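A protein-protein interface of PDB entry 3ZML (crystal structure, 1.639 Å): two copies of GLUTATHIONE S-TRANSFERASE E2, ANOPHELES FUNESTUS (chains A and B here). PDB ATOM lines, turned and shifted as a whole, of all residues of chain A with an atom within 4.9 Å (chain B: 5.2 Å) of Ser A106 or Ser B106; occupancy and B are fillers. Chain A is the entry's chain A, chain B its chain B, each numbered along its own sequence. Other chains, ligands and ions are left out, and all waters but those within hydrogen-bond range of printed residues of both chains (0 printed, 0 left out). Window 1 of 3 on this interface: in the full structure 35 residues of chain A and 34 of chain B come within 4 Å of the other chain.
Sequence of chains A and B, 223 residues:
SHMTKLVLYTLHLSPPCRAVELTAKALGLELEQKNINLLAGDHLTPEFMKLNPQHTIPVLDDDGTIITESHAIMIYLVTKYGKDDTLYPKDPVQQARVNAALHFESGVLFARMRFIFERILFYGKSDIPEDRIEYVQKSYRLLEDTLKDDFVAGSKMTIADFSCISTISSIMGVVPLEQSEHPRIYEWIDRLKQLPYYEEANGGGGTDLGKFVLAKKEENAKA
Leu A102 touches His B103, and with the chains exchanged His A103 touches Leu B102. His B103 touches its own counterpart, His A103. His A103 touches Ser B106, and with the chains exchanged Ser A106 touches His B103. Ser A106 touches Gly B107, and with the chains exchanged Gly A107 touches Ser B106. Positions printed for both chains: 71, 102, 103, 104, 105, 106, 107, 108, 110 and 111. Of the 13 pairs that touch across the chains among the printed residues, 13 have their exchanged pair printed and touching as well.
Ser A106 touches just these residues of chain B: His B103, Ser B106 and Gly B107. Of chain A, only His A103 (2.9 Å), Ser A106 (2.8 Å) and Gly A107 (3.4 Å) come within 4 Å of Ser B106. Of the printed residues of chain B, Leu A102 touches His B103. Printed residues of chain A within 4 Å of Gly B107: Ser A106 and Ala A111. Phe A110 touches none of the printed residues of chain B. The nearest printed residue of chain A that does not touch Gly B107 is Gly A107 (4.2 Å).
Of the 10 printed residues of chain A, 6 touch a printed residue of chain B. Hydrophobic or aromatic side chains of chain A within 4 Å of the printed part of chain B: His A71, Leu A102, His A103 and Ala A111.
The side-chain hydroxyl (OG) of Ser B106 is in hydrogen-bond range of the backbone carbonyl oxygen (O) of His B103 (3.4 Å). O of His A103 sits at hydrogen-bond distance from OG of Ser A106 (3.5 Å). A ring nitrogen (NE2) of His B71 is in hydrogen-bond range of the side-chain carboxylate (OE1) of Glu B105 (2.7 Å). O of Ser B106 lies within hydrogen-bond range of N of Ala B111 (3.4 Å). O of Ser A106 lies within hydrogen-bond range of N of Ala A111 (3.4 Å). A ring nitrogen (NE2) of His A71 lies within hydrogen-bond range of the side-chain carboxylate of Glu A105 (2.7 Å).
CE1 of His B103 touches O of Leu A102, 3.5 Å away. CB of His B71 touches NE2 of His A103, at 3.4 Å. O of Leu B102 touches CE1 of His A103, 3.6 Å away. Ser A106 touches Gly B107. Gly A107 touches Ser B106. Ala B111 touches Gly A107. Gly B107 touches Ala A111 (O to CB, 3.8 Å). Ala B111 touches Ala A111 (CB to CB, 3.7 Å).
ND1 of His A103 sits at hydrogen-bond distance from OG of Ser B106, 2.9 Å away. The side-chain hydroxyl of Ser A106 lies within hydrogen-bond range of the side-chain hydroxyl of Ser B106 (2.8 Å). A ring nitrogen (ND1) of His A71 lies within hydrogen-bond range of a ring nitrogen (ND1) of His B103 (3.5 Å). A ring nitrogen (ND1) of His B103 lies within hydrogen-bond range of the side-chain hydroxyl of Ser A106, 2.9 Å away. NE2 of His A103 sits at hydrogen-bond distance from NE2 of His B103 (3.3 Å).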
ATOM      1  N   HIS A  71      19.350  -2.291  21.390  1.00  0.00           N
ATOM      2  CA  HIS A  71      19.523  -3.125  22.583  1.00  0.00           C
ATOM      3  C   HIS A  71      19.556  -2.266  23.818  1.00  0.00           C
ATOM      4  O   HIS A  71      18.903  -2.586  24.851  1.00  0.00           O
ATOM      5  CB  HIS A  71      20.782  -4.020  22.437  1.00  0.00           C
ATOM      6  CG  HIS A  71      20.839  -4.772  21.134  1.00  0.00           C
ATOM      7  ND1 HIS A  71      21.348  -4.240  19.997  1.00  0.00           N
ATOM      8  CD2 HIS A  71      20.360  -6.013  20.788  1.00  0.00           C
ATOM      9  CE1 HIS A  71      21.241  -5.138  18.976  1.00  0.00           C
ATOM     10  NE2 HIS A  71      20.611  -6.208  19.450  1.00  0.00           N
ATOM     11  N   LEU A 102      21.652 -10.965  23.579  1.00  0.00           N
ATOM     12  CA  LEU A 102      21.584  -9.687  22.926  1.00  0.00           C
ATOM     13  C   LEU A 102      22.811  -9.428  22.027  1.00  0.00           C
ATOM     14  O   LEU A 102      22.715  -8.964  20.884  1.00  0.00           O
ATOM     15  CB  LEU A 102      21.378  -8.537  23.908  1.00  0.00           C
ATOM     16  CG  LEU A 102      20.000  -8.518  24.600  1.00  0.00           C
ATOM     17  CD1 LEU A 102      20.009  -7.584  25.808  1.00  0.00           C
ATOM     18  CD2 LEU A 102      18.930  -8.116  23.592  1.00  0.00           C
ATOM     19  N   HIS A 103      24.002  -9.679  22.588  1.00  0.00           N
ATOM     20  CA  HIS A 103      25.237  -9.522  21.792  1.00  0.00           C
ATOM     21  C   HIS A 103      25.465 -10.583  20.755  1.00  0.00           C
ATOM     22  O   HIS A 103      26.080 -10.328  19.702  1.00  0.00           O
ATOM     23  CB  HIS A 103      26.421  -9.417  22.745  1.00  0.00           C
ATOM     24  CG  HIS A 103      26.550  -8.068  23.387  1.00  0.00           C
ATOM     25  ND1 HIS A 103      27.130  -6.999  22.757  1.00  0.00           N
ATOM     26  CD2 HIS A 103      26.251  -7.637  24.683  1.00  0.00           C
ATOM     27  CE1 HIS A 103      27.080  -5.926  23.573  1.00  0.00           C
ATOM     28  NE2 HIS A 103      26.537  -6.314  24.741  1.00  0.00           N
ATOM     29  N   PHE A 104      24.896 -11.774  20.954  1.00  0.00           N
ATOM     30  CA  PHE A 104      24.897 -12.740  19.906  1.00  0.00           C
ATOM     31  C   PHE A 104      24.018 -12.166  18.735  1.00  0.00           C
ATOM     32  O   PHE A 104      24.409 -12.297  17.570  1.00  0.00           O
ATOM     33  CB  PHE A 104      24.237 -14.021  20.465  1.00  0.00           C
ATOM     34  CG  PHE A 104      23.973 -15.071  19.395  1.00  0.00           C
ATOM     35  CD1 PHE A 104      25.029 -15.716  18.769  1.00  0.00           C
ATOM     36  CD2 PHE A 104      22.635 -15.406  19.024  1.00  0.00           C
ATOM     37  CE1 PHE A 104      24.785 -16.652  17.741  1.00  0.00           C
ATOM     38  CE2 PHE A 104      22.402 -16.373  17.999  1.00  0.00           C
ATOM     39  CZ  PHE A 104      23.486 -16.996  17.352  1.00  0.00           C
ATOM     40  N   GLU A 105      22.879 -11.546  19.050  1.00  0.00           N
ATOM     41  CA  GLU A 105      22.047 -10.954  17.984  1.00  0.00           C
ATOM     42  C   GLU A 105      22.824  -9.832  17.218  1.00  0.00           C
ATOM     43  O   GLU A 105      22.847  -9.844  15.976  1.00  0.00           O
ATOM     44  CB  GLU A 105      20.731 -10.420  18.547  1.00  0.00           C
ATOM     45  CG  GLU A 105      19.730 -10.139  17.397  1.00  0.00           C
ATOM     46  CD  GLU A 105      19.912  -8.786  16.712  1.00  0.00           C
ATOM     47  OE1 GLU A 105      20.533  -7.879  17.328  1.00  0.00           O
ATOM     48  OE2 GLU A 105      19.338  -8.594  15.593  1.00  0.00           O
ATOM     49  N   SER A 106      23.467  -8.892  17.965  1.00  0.00           N
ATOM     50  CA  SER A 106      24.134  -7.813  17.258  1.00  0.00           C
ATOM     51  C   SER A 106      25.380  -8.305  16.518  1.00  0.00           C
ATOM     52  O   SER A 106      25.597  -7.918  15.335  1.00  0.00           O
ATOM     53  CB  SER A 106      24.417  -6.587  18.196  1.00  0.00           C
ATOM     54  OG  SER A 106      25.236  -6.985  19.248  1.00  0.00           O
ATOM     55  N   GLY A 107      26.130  -9.163  17.185  1.00  0.00           N
ATOM     56  CA  GLY A 107      27.414  -9.541  16.658  1.00  0.00           C
ATOM     57  C   GLY A 107      27.347 -10.608  15.581  1.00  0.00           C
ATOM     58  O   GLY A 107      28.281 -10.711  14.827  1.00  0.00           O
ATOM     59  N   VAL A 108      26.344 -11.479  15.615  1.00  0.00           N
ATOM     60  CA  VAL A 108      26.274 -12.626  14.740  1.00  0.00           C
ATOM     61  C   VAL A 108      25.006 -12.516  13.867  1.00  0.00           C
ATOM     62  O   VAL A 108      25.142 -12.420  12.659  1.00  0.00           O
ATOM     63  CB  VAL A 108      26.272 -13.986  15.491  1.00  0.00           C
ATOM     64  CG1 VAL A 108      26.182 -15.153  14.552  1.00  0.00           C
ATOM     65  CG2 VAL A 108      27.598 -14.138  16.263  1.00  0.00           C
ATOM     66  N   PHE A 110      22.463 -10.234  13.323  1.00  0.00           N
ATOM     67  CA  PHE A 110      22.235  -8.999  12.586  1.00  0.00           C
ATOM     68  C   PHE A 110      23.403  -8.677  11.699  1.00  0.00           C
ATOM     69  O   PHE A 110      23.243  -8.275  10.531  1.00  0.00           O
ATOM     70  CB  PHE A 110      21.869  -7.851  13.517  1.00  0.00           C
ATOM     71  CG  PHE A 110      21.624  -6.532  12.788  1.00  0.00           C
ATOM     72  CD1 PHE A 110      20.366  -6.256  12.257  1.00  0.00           C
ATOM     73  CD2 PHE A 110      22.652  -5.586  12.634  1.00  0.00           C
ATOM     74  CE1 PHE A 110      20.114  -5.054  11.589  1.00  0.00           C
ATOM     75  CE2 PHE A 110      22.388  -4.350  11.994  1.00  0.00           C
ATOM     76  CZ  PHE A 110      21.115  -4.117  11.416  1.00  0.00           C
ATOM     77  N   ALA A 111      24.637  -8.787  12.229  1.00  0.00           N
ATOM     78  CA  ALA A 111      25.757  -8.442  11.411  1.00  0.00           C
ATOM     79  C   ALA A 111      25.832  -9.232  10.116  1.00  0.00           C
ATOM     80  O   ALA A 111      26.168  -8.686   9.055  1.00  0.00           O
ATOM     81  CB  ALA A 111      27.049  -8.558  12.238  1.00  0.00           C
ATOM     82  N   HIS B  71      30.966  -9.223  26.678  1.00  0.00           N
ATOM     83  CA  HIS B  71      30.265  -8.074  27.208  1.00  0.00           C
ATOM     84  C   HIS B  71      29.367  -8.414  28.441  1.00  0.00           C
ATOM     85  O   HIS B  71      29.355  -7.718  29.430  1.00  0.00           O
ATOM     86  CB  HIS B  71      29.453  -7.394  26.103  1.00  0.00           C
ATOM     87  CG  HIS B  71      30.217  -7.172  24.832  1.00  0.00           C
ATOM     88  ND1 HIS B  71      30.333  -8.140  23.862  1.00  0.00           N
ATOM     89  CD2 HIS B  71      30.865  -6.088  24.355  1.00  0.00           C
ATOM     90  CE1 HIS B  71      31.052  -7.667  22.867  1.00  0.00           C
ATOM     91  NE2 HIS B  71      31.383  -6.428  23.134  1.00  0.00           N
ATOM     92  N   LEU B 102      28.876  -0.710  23.651  1.00  0.00           N
ATOM     93  CA  LEU B 102      29.196  -2.128  23.703  1.00  0.00           C
ATOM     94  C   LEU B 102      28.638  -2.892  22.472  1.00  0.00           C
ATOM     95  O   LEU B 102      29.325  -3.746  21.892  1.00  0.00           O
ATOM     96  CB  LEU B 102      28.566  -2.784  25.015  1.00  0.00           C
ATOM     97  CG  LEU B 102      29.313  -2.434  26.387  1.00  0.00           C
ATOM     98  CD1 LEU B 102      28.482  -2.774  27.613  1.00  0.00           C
ATOM     99  CD2 LEU B 102      30.719  -3.036  26.467  1.00  0.00           C
ATOM    100  N   HIS B 103      27.386  -2.597  22.114  1.00  0.00           N
ATOM    101  CA  HIS B 103      26.776  -3.237  20.941  1.00  0.00           C
ATOM    102  C   HIS B 103      27.343  -2.692  19.652  1.00  0.00           C
ATOM    103  O   HIS B 103      27.336  -3.399  18.624  1.00  0.00           O
ATOM    104  CB  HIS B 103      25.259  -3.115  20.925  1.00  0.00           C
ATOM    105  CG  HIS B 103      24.605  -4.092  21.861  1.00  0.00           C
ATOM    106  ND1 HIS B 103      24.304  -5.353  21.492  1.00  0.00           N
ATOM    107  CD2 HIS B 103      24.221  -3.962  23.163  1.00  0.00           C
ATOM    108  CE1 HIS B 103      23.814  -6.026  22.524  1.00  0.00           C
ATOM    109  NE2 HIS B 103      23.691  -5.161  23.557  1.00  0.00           N
ATOM    110  N   PHE B 104      27.815  -1.430  19.653  1.00  0.00           N
ATOM    111  CA  PHE B 104      28.597  -0.963  18.521  1.00  0.00           C
ATOM    112  C   PHE B 104      29.875  -1.826  18.384  1.00  0.00           C
ATOM    113  O   PHE B 104      30.272  -2.208  17.244  1.00  0.00           O
ATOM    114  CB  PHE B 104      28.948   0.535  18.699  1.00  0.00           C
ATOM    115  CG  PHE B 104      29.905   1.058  17.642  1.00  0.00           C
ATOM    116  CD1 PHE B 104      29.437   1.287  16.328  1.00  0.00           C
ATOM    117  CD2 PHE B 104      31.201   1.327  17.948  1.00  0.00           C
ATOM    118  CE1 PHE B 104      30.266   1.787  15.351  1.00  0.00           C
ATOM    119  CE2 PHE B 104      32.074   1.813  16.970  1.00  0.00           C
ATOM    120  CZ  PHE B 104      31.605   2.060  15.674  1.00  0.00           C
ATOM    121  N   GLU B 105      30.540  -2.156  19.482  1.00  0.00           N
ATOM    122  CA  GLU B 105      31.732  -2.970  19.365  1.00  0.00           C
ATOM    123  C   GLU B 105      31.401  -4.386  18.780  1.00  0.00           C
ATOM    124  O   GLU B 105      32.042  -4.878  17.865  1.00  0.00           O
ATOM    125  CB  GLU B 105      32.477  -3.070  20.707  1.00  0.00           C
ATOM    126  CG  GLU B 105      33.860  -3.714  20.568  1.00  0.00           C
ATOM    127  CD  GLU B 105      33.899  -5.247  20.551  1.00  0.00           C
ATOM    128  OE1 GLU B 105      32.901  -5.904  20.968  1.00  0.00           O
ATOM    129  OE2 GLU B 105      34.938  -5.826  20.146  1.00  0.00           O
ATOM    130  N   SER B 106      30.364  -5.024  19.290  1.00  0.00           N
ATOM    131  CA  SER B 106      30.079  -6.368  18.823  1.00  0.00           C
ATOM    132  C   SER B 106      29.491  -6.373  17.420  1.00  0.00           C
ATOM    133  O   SER B 106      29.898  -7.198  16.574  1.00  0.00           O
ATOM    134  CB  SER B 106      29.160  -7.119  19.786  1.00  0.00           C
ATOM    135  OG  SER B 106      27.927  -6.487  20.007  1.00  0.00           O
ATOM    136  N   GLY B 107      28.569  -5.461  17.158  1.00  0.00           N
ATOM    137  CA  GLY B 107      27.853  -5.475  15.908  1.00  0.00           C
ATOM    138  C   GLY B 107      28.646  -4.877  14.752  1.00  0.00           C
ATOM    139  O   GLY B 107      28.393  -5.215  13.585  1.00  0.00           O
ATOM    140  N   VAL B 108      29.580  -3.973  15.052  1.00  0.00           N
ATOM    141  CA  VAL B 108      30.316  -3.208  14.010  1.00  0.00           C
ATOM    142  C   VAL B 108      31.840  -3.464  14.068  1.00  0.00           C
ATOM    143  O   VAL B 108      32.411  -4.058  13.159  1.00  0.00           O
ATOM    144  CB  VAL B 108      30.026  -1.697  14.020  1.00  0.00           C
ATOM    145  CG1 VAL B 108      30.828  -0.977  12.923  1.00  0.00           C
ATOM    146  CG2 VAL B 108      28.498  -1.404  13.801  1.00  0.00           C
ATOM    147  N   LEU B 109      32.484  -3.085  15.161  1.00  0.00           N
ATOM    148  CA  LEU B 109      33.954  -3.193  15.153  1.00  0.00           C
ATOM    149  C   LEU B 109      34.452  -4.658  15.093  1.00  0.00           C
ATOM    150  O   LEU B 109      35.195  -5.024  14.201  1.00  0.00           O
ATOM    151  CB  LEU B 109      34.619  -2.455  16.371  1.00  0.00           C
ATOM    152  CG  LEU B 109      34.279  -0.979  16.501  1.00  0.00           C
ATOM    153  CD1 LEU B 109      34.931  -0.474  17.795  1.00  0.00           C
ATOM    154  CD2 LEU B 109      34.869  -0.126  15.348  1.00  0.00           C
ATOM    155  N   PHE B 110      33.939  -5.486  15.977  1.00  0.00           N
ATOM    156  CA  PHE B 110      34.402  -6.886  16.088  1.00  0.00           C
ATOM    157  C   PHE B 110      33.894  -7.673  14.893  1.00  0.00           C
ATOM    158  O   PHE B 110      34.639  -8.397  14.253  1.00  0.00           O
ATOM    159  CB  PHE B 110      33.910  -7.548  17.355  1.00  0.00           C
ATOM    160  CG  PHE B 110      34.382  -8.985  17.491  1.00  0.00           C
ATOM    161  CD1 PHE B 110      35.676  -9.272  17.962  1.00  0.00           C
ATOM    162  CD2 PHE B 110      33.585 -10.058  17.107  1.00  0.00           C
ATOM    163  CE1 PHE B 110      36.119 -10.645  18.070  1.00  0.00           C
ATOM    164  CE2 PHE B 110      34.001 -11.433  17.234  1.00  0.00           C
ATOM    165  CZ  PHE B 110      35.275 -11.727  17.728  1.00  0.00           C
ATOM    166  N   ALA B 111      32.597  -7.513  14.579  1.00  0.00           N
ATOM    167  CA  ALA B 111      32.076  -8.251  13.453  1.00  0.00           C
ATOM    168  C   ALA B 111      32.864  -8.068  12.163  1.00  0.00           C
ATOM    169  O   ALA B 111      33.130  -9.041  11.434  1.00  0.00           O
ATOM    170  CB  ALA B 111      30.557  -7.927  13.200  1.00  0.00           C
